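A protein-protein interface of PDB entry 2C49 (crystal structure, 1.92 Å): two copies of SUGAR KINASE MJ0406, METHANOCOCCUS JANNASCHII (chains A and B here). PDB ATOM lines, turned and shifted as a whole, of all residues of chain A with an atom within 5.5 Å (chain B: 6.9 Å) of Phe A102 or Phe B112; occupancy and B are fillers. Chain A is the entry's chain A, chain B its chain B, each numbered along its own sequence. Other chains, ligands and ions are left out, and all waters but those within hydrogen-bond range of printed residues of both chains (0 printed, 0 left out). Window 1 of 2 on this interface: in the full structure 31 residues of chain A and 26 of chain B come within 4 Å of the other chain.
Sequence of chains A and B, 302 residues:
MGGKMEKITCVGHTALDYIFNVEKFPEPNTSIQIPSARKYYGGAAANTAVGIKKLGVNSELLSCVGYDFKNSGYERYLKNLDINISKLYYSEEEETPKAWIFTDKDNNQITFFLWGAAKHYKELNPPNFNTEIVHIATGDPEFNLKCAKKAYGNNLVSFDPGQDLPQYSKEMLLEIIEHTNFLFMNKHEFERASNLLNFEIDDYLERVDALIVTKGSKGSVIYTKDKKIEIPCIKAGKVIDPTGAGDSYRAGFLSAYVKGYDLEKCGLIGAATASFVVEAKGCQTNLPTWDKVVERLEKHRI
NE1 of Trp A100 sits close to NE1 of Trp B100, 3.4 Å away.
The backbone carbonyl oxygen of Thr B111 is in hydrogen-bond range of the backbone NH of Ile A32.
The backbone NH (N) of Ile A34 is in hydrogen-bond range of the backbone carbonyl oxygen (O) of Phe B113.
The backbone NH (N) of Phe B113 sits at hydrogen-bond distance from the backbone carbonyl oxygen (O) of Ile A32, at 2.8 Å.
Of the 17 printed residues of chain A, 8 touch a printed residue of chain B.
Hydrophobic or aromatic side chains of chain A that line the printed part of chain B: Phe A20, Pro A26, Ile A34, Trp A100, Phe A102 and Phe A112.
Printed residues of chain B that touch a printed residue of chain A: Trp B100, Phe B102, Ile B110, Thr B111, Phe B112, Phe B113 and Leu B114.
Among the printed residues, no Asp or Glu carboxylate lies within 4 Å of a Lys or Arg side-chain nitrogen of the other chain.
Trp A100 touches its own counterpart, Trp B100.
Phe A102 touches Phe B112, and with the chains exchanged Phe A112 touches Phe B102.
Positions printed for both chains: 100, 101, 102, 110, 111 and 112.
Of the 12 pairs that touch across the chains among the printed residues, 3 have their exchanged pair printed and touching as well.
Printed residues of chain B within 4 Å of Trp A100: Trp B100.
Phe A102 touches just one residue of chain B: Phe B112.
Phe B112 touches just these residues of chain A: Pro A26, Ile A32 and Phe A102.
Of the printed residues of chain A, Leu B114 touches Ile A34 (3.4 Å).
The nearest printed residue of chain B that does not touch Pro A26 is Thr B111 (6.3 Å).
N of Thr A103 is in hydrogen-bond range of O of Phe A20, 2.7 Å away.
The backbone carbonyl oxygen of Ile A101 is in hydrogen-bond range of the backbone NH of Phe A20.
The backbone NH of Leu B114 sits at hydrogen-bond distance from the backbone carbonyl oxygen of Lys B98, at 2.8 Å.
The backbone NH (N) of Trp A100 sits at hydrogen-bond distance from the backbone carbonyl oxygen (O) of Phe A112 (2.8 Å).
N of Trp B100 is in hydrogen-bond range of O of Phe B112, 2.8 Å away.
The backbone NH (N) of Phe A102 lies within hydrogen-bond range of the backbone carbonyl oxygen (O) of Ile A110 (3.0 Å).
Phe A20 touches Trp B100.
Ile B110 touches Pro A26.
Pro A26 touches Phe B112 (CG to CZ, 3.6 Å).
O of Thr B111 touches CA of Ser A31, at 3.3 Å.
O of Ile A32 touches CA of Phe B112, 3.4 Å away.
Leu B114 touches Ile A34 (CD1 to O, 3.4 Å).
CE2 of Phe B112 touches CE2 of Phe A102 (3.3 Å).
Phe A112 touches Phe B102 (CD2 to CD2, 3.4 Å).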
ATOM      1  N   PHE A  20       2.908  23.886  15.737  1.00  0.00           N
ATOM      2  CA  PHE A  20       3.444  25.079  15.076  1.00  0.00           C
ATOM      3  C   PHE A  20       3.762  26.221  16.060  1.00  0.00           C
ATOM      4  O   PHE A  20       3.009  26.474  17.015  1.00  0.00           O
ATOM      5  CB  PHE A  20       2.489  25.652  14.007  1.00  0.00           C
ATOM      6  CG  PHE A  20       1.863  24.631  13.096  1.00  0.00           C
ATOM      7  CD1 PHE A  20       0.626  24.072  13.408  1.00  0.00           C
ATOM      8  CD2 PHE A  20       2.480  24.275  11.906  1.00  0.00           C
ATOM      9  CE1 PHE A  20       0.033  23.149  12.569  1.00  0.00           C
ATOM     10  CE2 PHE A  20       1.900  23.361  11.058  1.00  0.00           C
ATOM     11  CZ  PHE A  20       0.676  22.789  11.387  1.00  0.00           C
ATOM     12  N   VAL A  22       4.183  30.212  16.250  1.00  0.00           N
ATOM     13  CA  VAL A  22       3.820  31.487  15.647  1.00  0.00           C
ATOM     14  C   VAL A  22       4.190  32.581  16.651  1.00  0.00           C
ATOM     15  O   VAL A  22       4.329  32.308  17.843  1.00  0.00           O
ATOM     16  CB  VAL A  22       2.310  31.548  15.193  1.00  0.00           C
ATOM     17  CG1 VAL A  22       1.963  30.393  14.191  1.00  0.00           C
ATOM     18  CG2 VAL A  22       1.356  31.495  16.362  1.00  0.00           C
ATOM     19  N   PHE A  25      -1.077  34.536  17.398  1.00  0.00           N
ATOM     20  CA  PHE A  25      -2.134  33.763  16.755  1.00  0.00           C
ATOM     21  C   PHE A  25      -2.798  34.575  15.641  1.00  0.00           C
ATOM     22  O   PHE A  25      -3.056  35.765  15.822  1.00  0.00           O
ATOM     23  CB  PHE A  25      -3.202  33.407  17.779  1.00  0.00           C
ATOM     24  CG  PHE A  25      -2.705  32.578  18.928  1.00  0.00           C
ATOM     25  CD1 PHE A  25      -3.060  32.907  20.232  1.00  0.00           C
ATOM     26  CD2 PHE A  25      -1.934  31.429  18.698  1.00  0.00           C
ATOM     27  CE1 PHE A  25      -2.630  32.113  21.314  1.00  0.00           C
ATOM     28  CE2 PHE A  25      -1.502  30.635  19.756  1.00  0.00           C
ATOM     29  CZ  PHE A  25      -1.847  30.974  21.070  1.00  0.00           C
ATOM     30  N   PRO A  26      -3.093  33.946  14.502  1.00  0.00           N
ATOM     31  CA  PRO A  26      -3.715  34.652  13.368  1.00  0.00           C
ATOM     32  C   PRO A  26      -5.110  35.149  13.729  1.00  0.00           C
ATOM     33  O   PRO A  26      -5.820  34.506  14.513  1.00  0.00           O
ATOM     34  CB  PRO A  26      -3.834  33.556  12.314  1.00  0.00           C
ATOM     35  CG  PRO A  26      -3.896  32.331  13.109  1.00  0.00           C
ATOM     36  CD  PRO A  26      -2.885  32.526  14.204  1.00  0.00           C
ATOM     37  N   SER A  31      -4.235  34.719   6.253  1.00  0.00           N
ATOM     38  CA  SER A  31      -3.504  33.501   5.915  1.00  0.00           C
ATOM     39  C   SER A  31      -2.071  33.609   6.382  1.00  0.00           C
ATOM     40  O   SER A  31      -1.467  34.707   6.383  1.00  0.00           O
ATOM     41  CB  SER A  31      -3.523  33.227   4.401  1.00  0.00           C
ATOM     42  OG  SER A  31      -4.819  33.455   3.849  1.00  0.00           O
ATOM     43  N   ILE A  32      -1.535  32.458   6.773  1.00  0.00           N
ATOM     44  CA  ILE A  32      -0.167  32.350   7.231  1.00  0.00           C
ATOM     45  C   ILE A  32       0.479  31.188   6.445  1.00  0.00           C
ATOM     46  O   ILE A  32      -0.168  30.171   6.189  1.00  0.00           O
ATOM     47  CB  ILE A  32      -0.186  32.108   8.764  1.00  0.00           C
ATOM     48  CG1 ILE A  32      -0.424  33.427   9.518  1.00  0.00           C
ATOM     49  CG2 ILE A  32       1.089  31.433   9.275  1.00  0.00           C
ATOM     50  CD1 ILE A  32       0.626  34.521   9.276  1.00  0.00           C
ATOM     51  N   ILE A  34       3.335  28.298   6.575  1.00  0.00           N
ATOM     52  CA  ILE A  34       4.195  27.525   7.439  1.00  0.00           C
ATOM     53  C   ILE A  34       5.331  26.923   6.582  1.00  0.00           C
ATOM     54  O   ILE A  34       5.073  26.103   5.726  1.00  0.00           O
ATOM     55  CB  ILE A  34       3.365  26.387   8.125  1.00  0.00           C
ATOM     56  CG1 ILE A  34       2.219  26.954   8.993  1.00  0.00           C
ATOM     57  CG2 ILE A  34       4.287  25.401   8.897  1.00  0.00           C
ATOM     58  CD1 ILE A  34       2.672  27.941  10.094  1.00  0.00           C
ATOM     59  N   TRP A 100      -4.052  20.031  15.442  1.00  0.00           N
ATOM     60  CA  TRP A 100      -3.247  21.150  14.940  1.00  0.00           C
ATOM     61  C   TRP A 100      -3.052  22.086  16.122  1.00  0.00           C
ATOM     62  O   TRP A 100      -4.017  22.679  16.632  1.00  0.00           O
ATOM     63  CB  TRP A 100      -3.948  21.884  13.790  1.00  0.00           C
ATOM     64  CG  TRP A 100      -3.846  21.139  12.513  1.00  0.00           C
ATOM     65  CD1 TRP A 100      -3.000  21.407  11.469  1.00  0.00           C
ATOM     66  CD2 TRP A 100      -4.617  19.992  12.116  1.00  0.00           C
ATOM     67  NE1 TRP A 100      -3.200  20.513  10.440  1.00  0.00           N
ATOM     68  CE2 TRP A 100      -4.181  19.620  10.812  1.00  0.00           C
ATOM     69  CE3 TRP A 100      -5.653  19.252  12.712  1.00  0.00           C
ATOM     70  CZ2 TRP A 100      -4.698  18.519  10.129  1.00  0.00           C
ATOM     71  CZ3 TRP A 100      -6.177  18.160  12.017  1.00  0.00           C
ATOM     72  CH2 TRP A 100      -5.687  17.803  10.736  1.00  0.00           C
ATOM     73  N   ILE A 101      -1.800  22.206  16.548  1.00  0.00           N
ATOM     74  CA  ILE A 101      -1.441  22.880  17.793  1.00  0.00           C
ATOM     75  C   ILE A 101      -0.555  24.076  17.489  1.00  0.00           C
ATOM     76  O   ILE A 101       0.489  23.942  16.828  1.00  0.00           O
ATOM     77  CB  ILE A 101      -0.718  21.866  18.721  1.00  0.00           C
ATOM     78  CG1 ILE A 101      -1.663  20.679  19.012  1.00  0.00           C
ATOM     79  CG2 ILE A 101      -0.224  22.542  20.019  1.00  0.00           C
ATOM     80  CD1 ILE A 101      -0.985  19.444  19.574  1.00  0.00           C
ATOM     81  N   PHE A 102      -1.000  25.245  17.943  1.00  0.00           N
ATOM     82  CA  PHE A 102      -0.288  26.486  17.681  1.00  0.00           C
ATOM     83  C   PHE A 102       0.178  27.058  18.983  1.00  0.00           C
ATOM     84  O   PHE A 102      -0.590  27.137  19.918  1.00  0.00           O
ATOM     85  CB  PHE A 102      -1.174  27.477  16.931  1.00  0.00           C
ATOM     86  CG  PHE A 102      -1.640  26.947  15.632  1.00  0.00           C
ATOM     87  CD1 PHE A 102      -2.729  26.096  15.572  1.00  0.00           C
ATOM     88  CD2 PHE A 102      -0.964  27.261  14.469  1.00  0.00           C
ATOM     89  CE1 PHE A 102      -3.137  25.568  14.352  1.00  0.00           C
ATOM     90  CE2 PHE A 102      -1.377  26.737  13.264  1.00  0.00           C
ATOM     91  CZ  PHE A 102      -2.464  25.901  13.211  1.00  0.00           C
ATOM     92  N   THR A 103       1.455  27.415  19.024  1.00  0.00           N
ATOM     93  CA  THR A 103       2.079  27.995  20.185  1.00  0.00           C
ATOM     94  C   THR A 103       2.571  29.413  19.857  1.00  0.00           C
ATOM     95  O   THR A 103       3.363  29.592  18.937  1.00  0.00           O
ATOM     96  CB  THR A 103       3.274  27.119  20.614  1.00  0.00           C
ATOM     97  OG1 THR A 103       2.836  25.763  20.815  1.00  0.00           O
ATOM     98  CG2 THR A 103       3.750  27.546  21.963  1.00  0.00           C
ATOM     99  N   ASP A 104       2.119  30.405  20.618  1.00  0.00           N
ATOM    100  CA  ASP A 104       2.573  31.779  20.399  1.00  0.00           C
ATOM    101  C   ASP A 104       3.848  32.071  21.192  1.00  0.00           C
ATOM    102  O   ASP A 104       4.341  31.191  21.907  1.00  0.00           O
ATOM    103  CB  ASP A 104       1.441  32.803  20.615  1.00  0.00           C
ATOM    104  CG  ASP A 104       1.177  33.147  22.092  1.00  0.00           C
ATOM    105  OD1 ASP A 104       1.869  32.658  23.019  1.00  0.00           O
ATOM    106  OD2 ASP A 104       0.264  33.943  22.409  1.00  0.00           O
ATOM    107  N   ASN A 108       1.394  30.606  25.054  1.00  0.00           N
ATOM    108  CA  ASN A 108      -0.024  30.289  24.945  1.00  0.00           C
ATOM    109  C   ASN A 108      -0.210  29.320  23.772  1.00  0.00           C
ATOM    110  O   ASN A 108       0.555  29.363  22.802  1.00  0.00           O
ATOM    111  CB  ASN A 108      -0.838  31.566  24.721  1.00  0.00           C
ATOM    112  CG  ASN A 108      -0.648  32.579  25.846  1.00  0.00           C
ATOM    113  OD1 ASN A 108      -0.909  32.281  27.011  1.00  0.00           O
ATOM    114  ND2 ASN A 108      -0.184  33.779  25.500  1.00  0.00           N
ATOM    115  N   GLN A 109      -1.220  28.452  23.860  1.00  0.00           N
ATOM    116  CA  GLN A 109      -1.532  27.526  22.767  1.00  0.00           C
ATOM    117  C   GLN A 109      -3.026  27.483  22.424  1.00  0.00           C
ATOM    118  O   GLN A 109      -3.885  27.661  23.280  1.00  0.00           O
ATOM    119  CB  GLN A 109      -1.045  26.101  23.088  1.00  0.00           C
ATOM    120  CG  GLN A 109       0.472  25.979  23.390  1.00  0.00           C
ATOM    121  CD  GLN A 109       0.961  24.541  23.343  1.00  0.00           C
ATOM    122  OE1 GLN A 109       1.721  24.162  22.443  1.00  0.00           O
ATOM    123  NE2 GLN A 109       0.522  23.731  24.302  1.00  0.00           N
ATOM    124  N   ILE A 110      -3.324  27.256  21.158  1.00  0.00           N
ATOM    125  CA  ILE A 110      -4.683  26.985  20.742  1.00  0.00           C
ATOM    126  C   ILE A 110      -4.630  25.667  19.995  1.00  0.00           C
ATOM    127  O   ILE A 110      -3.606  25.323  19.421  1.00  0.00           O
ATOM    128  CB  ILE A 110      -5.261  28.127  19.865  1.00  0.00           C
ATOM    129  CG1 ILE A 110      -4.447  28.334  18.576  1.00  0.00           C
ATOM    130  CG2 ILE A 110      -5.326  29.448  20.667  1.00  0.00           C
ATOM    131  CD1 ILE A 110      -4.984  29.502  17.669  1.00  0.00           C
ATOM    132  N   THR A 111      -5.707  24.898  20.009  1.00  0.00           N
ATOM    133  CA  THR A 111      -5.651  23.694  19.194  1.00  0.00           C
ATOM    134  C   THR A 111      -6.951  23.503  18.462  1.00  0.00           C
ATOM    135  O   THR A 111      -8.000  24.016  18.873  1.00  0.00           O
ATOM    136  CB  THR A 111      -5.294  22.410  20.014  1.00  0.00           C
ATOM    137  OG1 THR A 111      -6.444  21.997  20.770  1.00  0.00           O
ATOM    138  CG2 THR A 111      -4.193  22.648  21.068  1.00  0.00           C
ATOM    139  N   PHE A 112      -6.841  22.761  17.368  1.00  0.00           N
ATOM    140  CA  PHE A 112      -7.960  22.295  16.576  1.00  0.00           C
ATOM    141  C   PHE A 112      -7.808  20.788  16.577  1.00  0.00           C
ATOM    142  O   PHE A 112      -6.726  20.293  16.294  1.00  0.00           O
ATOM    143  CB  PHE A 112      -7.845  22.861  15.155  1.00  0.00           C
ATOM    144  CG  PHE A 112      -7.778  24.377  15.091  1.00  0.00           C
ATOM    145  CD1 PHE A 112      -6.568  25.066  15.260  1.00  0.00           C
ATOM    146  CD2 PHE A 112      -8.911  25.113  14.841  1.00  0.00           C
ATOM    147  CE1 PHE A 112      -6.519  26.464  15.156  1.00  0.00           C
ATOM    148  CE2 PHE A 112      -8.864  26.497  14.737  1.00  0.00           C
ATOM    149  CZ  PHE A 112      -7.675  27.174  14.905  1.00  0.00           C
ATOM    150  N   LYS B  98       0.051  22.054   1.248  1.00  0.00           N
ATOM    151  CA  LYS B  98      -1.338  21.832   1.538  1.00  0.00           C
ATOM    152  C   LYS B  98      -1.866  23.089   2.204  1.00  0.00           C
ATOM    153  O   LYS B  98      -1.076  23.893   2.743  1.00  0.00           O
ATOM    154  CB  LYS B  98      -1.554  20.556   2.414  1.00  0.00           C
ATOM    155  CG  LYS B  98      -0.568  20.363   3.594  1.00  0.00           C
ATOM    156  CD  LYS B  98      -0.877  19.114   4.457  1.00  0.00           C
ATOM    157  CE  LYS B  98      -0.657  17.774   3.718  1.00  0.00           C
ATOM    158  NZ  LYS B  98       0.757  17.465   3.373  1.00  0.00           N
ATOM    159  N   ALA B  99      -3.174  23.293   2.108  1.00  0.00           N
ATOM    160  CA  ALA B  99      -3.827  24.393   2.863  1.00  0.00           C
ATOM    161  C   ALA B  99      -4.768  23.778   3.890  1.00  0.00           C
ATOM    162  O   ALA B  99      -5.575  22.906   3.554  1.00  0.00           O
ATOM    163  CB  ALA B  99      -4.576  25.322   1.928  1.00  0.00           C
ATOM    164  N   TRP B 100      -4.617  24.189   5.150  1.00  0.00           N
ATOM    165  CA  TRP B 100      -5.548  23.814   6.197  1.00  0.00           C
ATOM    166  C   TRP B 100      -6.446  25.019   6.400  1.00  0.00           C
ATOM    167  O   TRP B 100      -5.981  26.071   6.840  1.00  0.00           O
ATOM    168  CB  TRP B 100      -4.806  23.497   7.485  1.00  0.00           C
ATOM    169  CG  TRP B 100      -3.942  22.275   7.374  1.00  0.00           C
ATOM    170  CD1 TRP B 100      -4.346  21.011   7.089  1.00  0.00           C
ATOM    171  CD2 TRP B 100      -2.526  22.221   7.555  1.00  0.00           C
ATOM    172  NE1 TRP B 100      -3.262  20.162   7.066  1.00  0.00           N
ATOM    173  CE2 TRP B 100      -2.131  20.877   7.367  1.00  0.00           C
ATOM    174  CE3 TRP B 100      -1.543  23.179   7.868  1.00  0.00           C
ATOM    175  CZ2 TRP B 100      -0.805  20.460   7.491  1.00  0.00           C
ATOM    176  CZ3 TRP B 100      -0.219  22.766   7.997  1.00  0.00           C
ATOM    177  CH2 TRP B 100       0.142  21.422   7.800  1.00  0.00           C
ATOM    178  N   ILE B 101      -7.730  24.865   6.071  1.00  0.00           N
ATOM    179  CA  ILE B 101      -8.645  26.001   6.017  1.00  0.00           C
ATOM    180  C   ILE B 101      -9.735  25.871   7.054  1.00  0.00           C
ATOM    181  O   ILE B 101     -10.582  24.987   6.975  1.00  0.00           O
ATOM    182  CB  ILE B 101      -9.267  26.141   4.646  1.00  0.00           C
ATOM    183  CG1 ILE B 101      -8.184  26.146   3.547  1.00  0.00           C
ATOM    184  CG2 ILE B 101     -10.166  27.415   4.612  1.00  0.00           C
ATOM    185  CD1 ILE B 101      -8.753  25.932   2.130  1.00  0.00           C
ATOM    186  N   PHE B 102      -9.704  26.767   8.029  1.00  0.00           N
ATOM    187  CA  PHE B 102     -10.635  26.690   9.148  1.00  0.00           C
ATOM    188  C   PHE B 102     -11.653  27.791   8.938  1.00  0.00           C
ATOM    189  O   PHE B 102     -11.283  28.956   8.772  1.00  0.00           O
ATOM    190  CB  PHE B 102      -9.879  26.884  10.480  1.00  0.00           C
ATOM    191  CG  PHE B 102      -8.904  25.809  10.770  1.00  0.00           C
ATOM    192  CD1 PHE B 102      -7.573  25.908  10.338  1.00  0.00           C
ATOM    193  CD2 PHE B 102      -9.309  24.668  11.459  1.00  0.00           C
ATOM    194  CE1 PHE B 102      -6.663  24.884  10.598  1.00  0.00           C
ATOM    195  CE2 PHE B 102      -8.406  23.631  11.735  1.00  0.00           C
ATOM    196  CZ  PHE B 102      -7.084  23.737  11.297  1.00  0.00           C
ATOM    197  N   ILE B 110      -9.652  31.194   8.437  1.00  0.00           N
ATOM    198  CA  ILE B 110      -8.229  31.323   8.727  1.00  0.00           C
ATOM    199  C   ILE B 110      -7.545  30.179   8.004  1.00  0.00           C
ATOM    200  O   ILE B 110      -7.942  29.031   8.169  1.00  0.00           O
ATOM    201  CB  ILE B 110      -7.944  31.278  10.259  1.00  0.00           C
ATOM    202  CG1 ILE B 110      -8.434  32.563  10.956  1.00  0.00           C
ATOM    203  CG2 ILE B 110      -6.447  31.145  10.524  1.00  0.00           C
ATOM    204  CD1 ILE B 110      -8.242  32.537  12.505  1.00  0.00           C
ATOM    205  N   THR B 111      -6.557  30.499   7.183  1.00  0.00           N
ATOM    206  CA  THR B 111      -5.873  29.513   6.354  1.00  0.00           C
ATOM    207  C   THR B 111      -4.416  29.385   6.770  1.00  0.00           C
ATOM    208  O   THR B 111      -3.702  30.379   6.933  1.00  0.00           O
ATOM    209  CB  THR B 111      -6.013  29.936   4.881  1.00  0.00           C
ATOM    210  OG1 THR B 111      -7.398  29.883   4.523  1.00  0.00           O
ATOM    211  CG2 THR B 111      -5.327  28.935   3.910  1.00  0.00           C
ATOM    212  N   PHE B 112      -3.975  28.159   6.971  1.00  0.00           N
ATOM    213  CA  PHE B 112      -2.558  27.886   7.161  1.00  0.00           C
ATOM    214  C   PHE B 112      -2.092  27.153   5.916  1.00  0.00           C
ATOM    215  O   PHE B 112      -2.582  26.070   5.640  1.00  0.00           O
ATOM    216  CB  PHE B 112      -2.329  27.029   8.417  1.00  0.00           C
ATOM    217  CG  PHE B 112      -2.846  27.674   9.681  1.00  0.00           C
ATOM    218  CD1 PHE B 112      -4.105  27.362  10.171  1.00  0.00           C
ATOM    219  CD2 PHE B 112      -2.082  28.611  10.354  1.00  0.00           C
ATOM    220  CE1 PHE B 112      -4.589  27.960  11.300  1.00  0.00           C
ATOM    221  CE2 PHE B 112      -2.578  29.234  11.493  1.00  0.00           C
ATOM    222  CZ  PHE B 112      -3.824  28.900  11.970  1.00  0.00           C
ATOM    223  N   PHE B 113      -1.185  27.777   5.157  1.00  0.00           N
ATOM    224  CA  PHE B 113      -0.539  27.117   4.025  1.00  0.00           C
ATOM    225  C   PHE B 113       0.845  26.557   4.367  1.00  0.00           C
ATOM    226  O   PHE B 113       1.753  27.276   4.824  1.00  0.00           O
ATOM    227  CB  PHE B 113      -0.437  28.043   2.815  1.00  0.00           C
ATOM    228  CG  PHE B 113       0.008  27.349   1.572  1.00  0.00           C
ATOM    229  CD1 PHE B 113      -0.810  26.397   0.953  1.00  0.00           C
ATOM    230  CD2 PHE B 113       1.240  27.651   0.991  1.00  0.00           C
ATOM    231  CE1 PHE B 113      -0.404  25.757  -0.233  1.00  0.00           C
ATOM    232  CE2 PHE B 113       1.654  26.996  -0.184  1.00  0.00           C
ATOM    233  CZ  PHE B 113       0.824  26.050  -0.787  1.00  0.00           C
ATOM    234  N   LEU B 114       0.988  25.263   4.126  1.00  0.00           N
ATOM    235  CA  LEU B 114       2.250  24.575   4.341  1.00  0.00           C
ATOM    236  C   LEU B 114       3.044  24.718   3.053  1.00  0.00           C
ATOM    237  O   LEU B 114       2.614  24.257   1.987  1.00  0.00           O
ATOM    238  CB  LEU B 114       2.020  23.104   4.735  1.00  0.00           C
ATOM    239  CG  LEU B 114       3.282  22.234   4.833  1.00  0.00           C
ATOM    240  CD1 LEU B 114       4.317  22.828   5.848  1.00  0.00           C
ATOM    241  CD2 LEU B 114       2.934  20.753   5.151  1.00  0.00           C
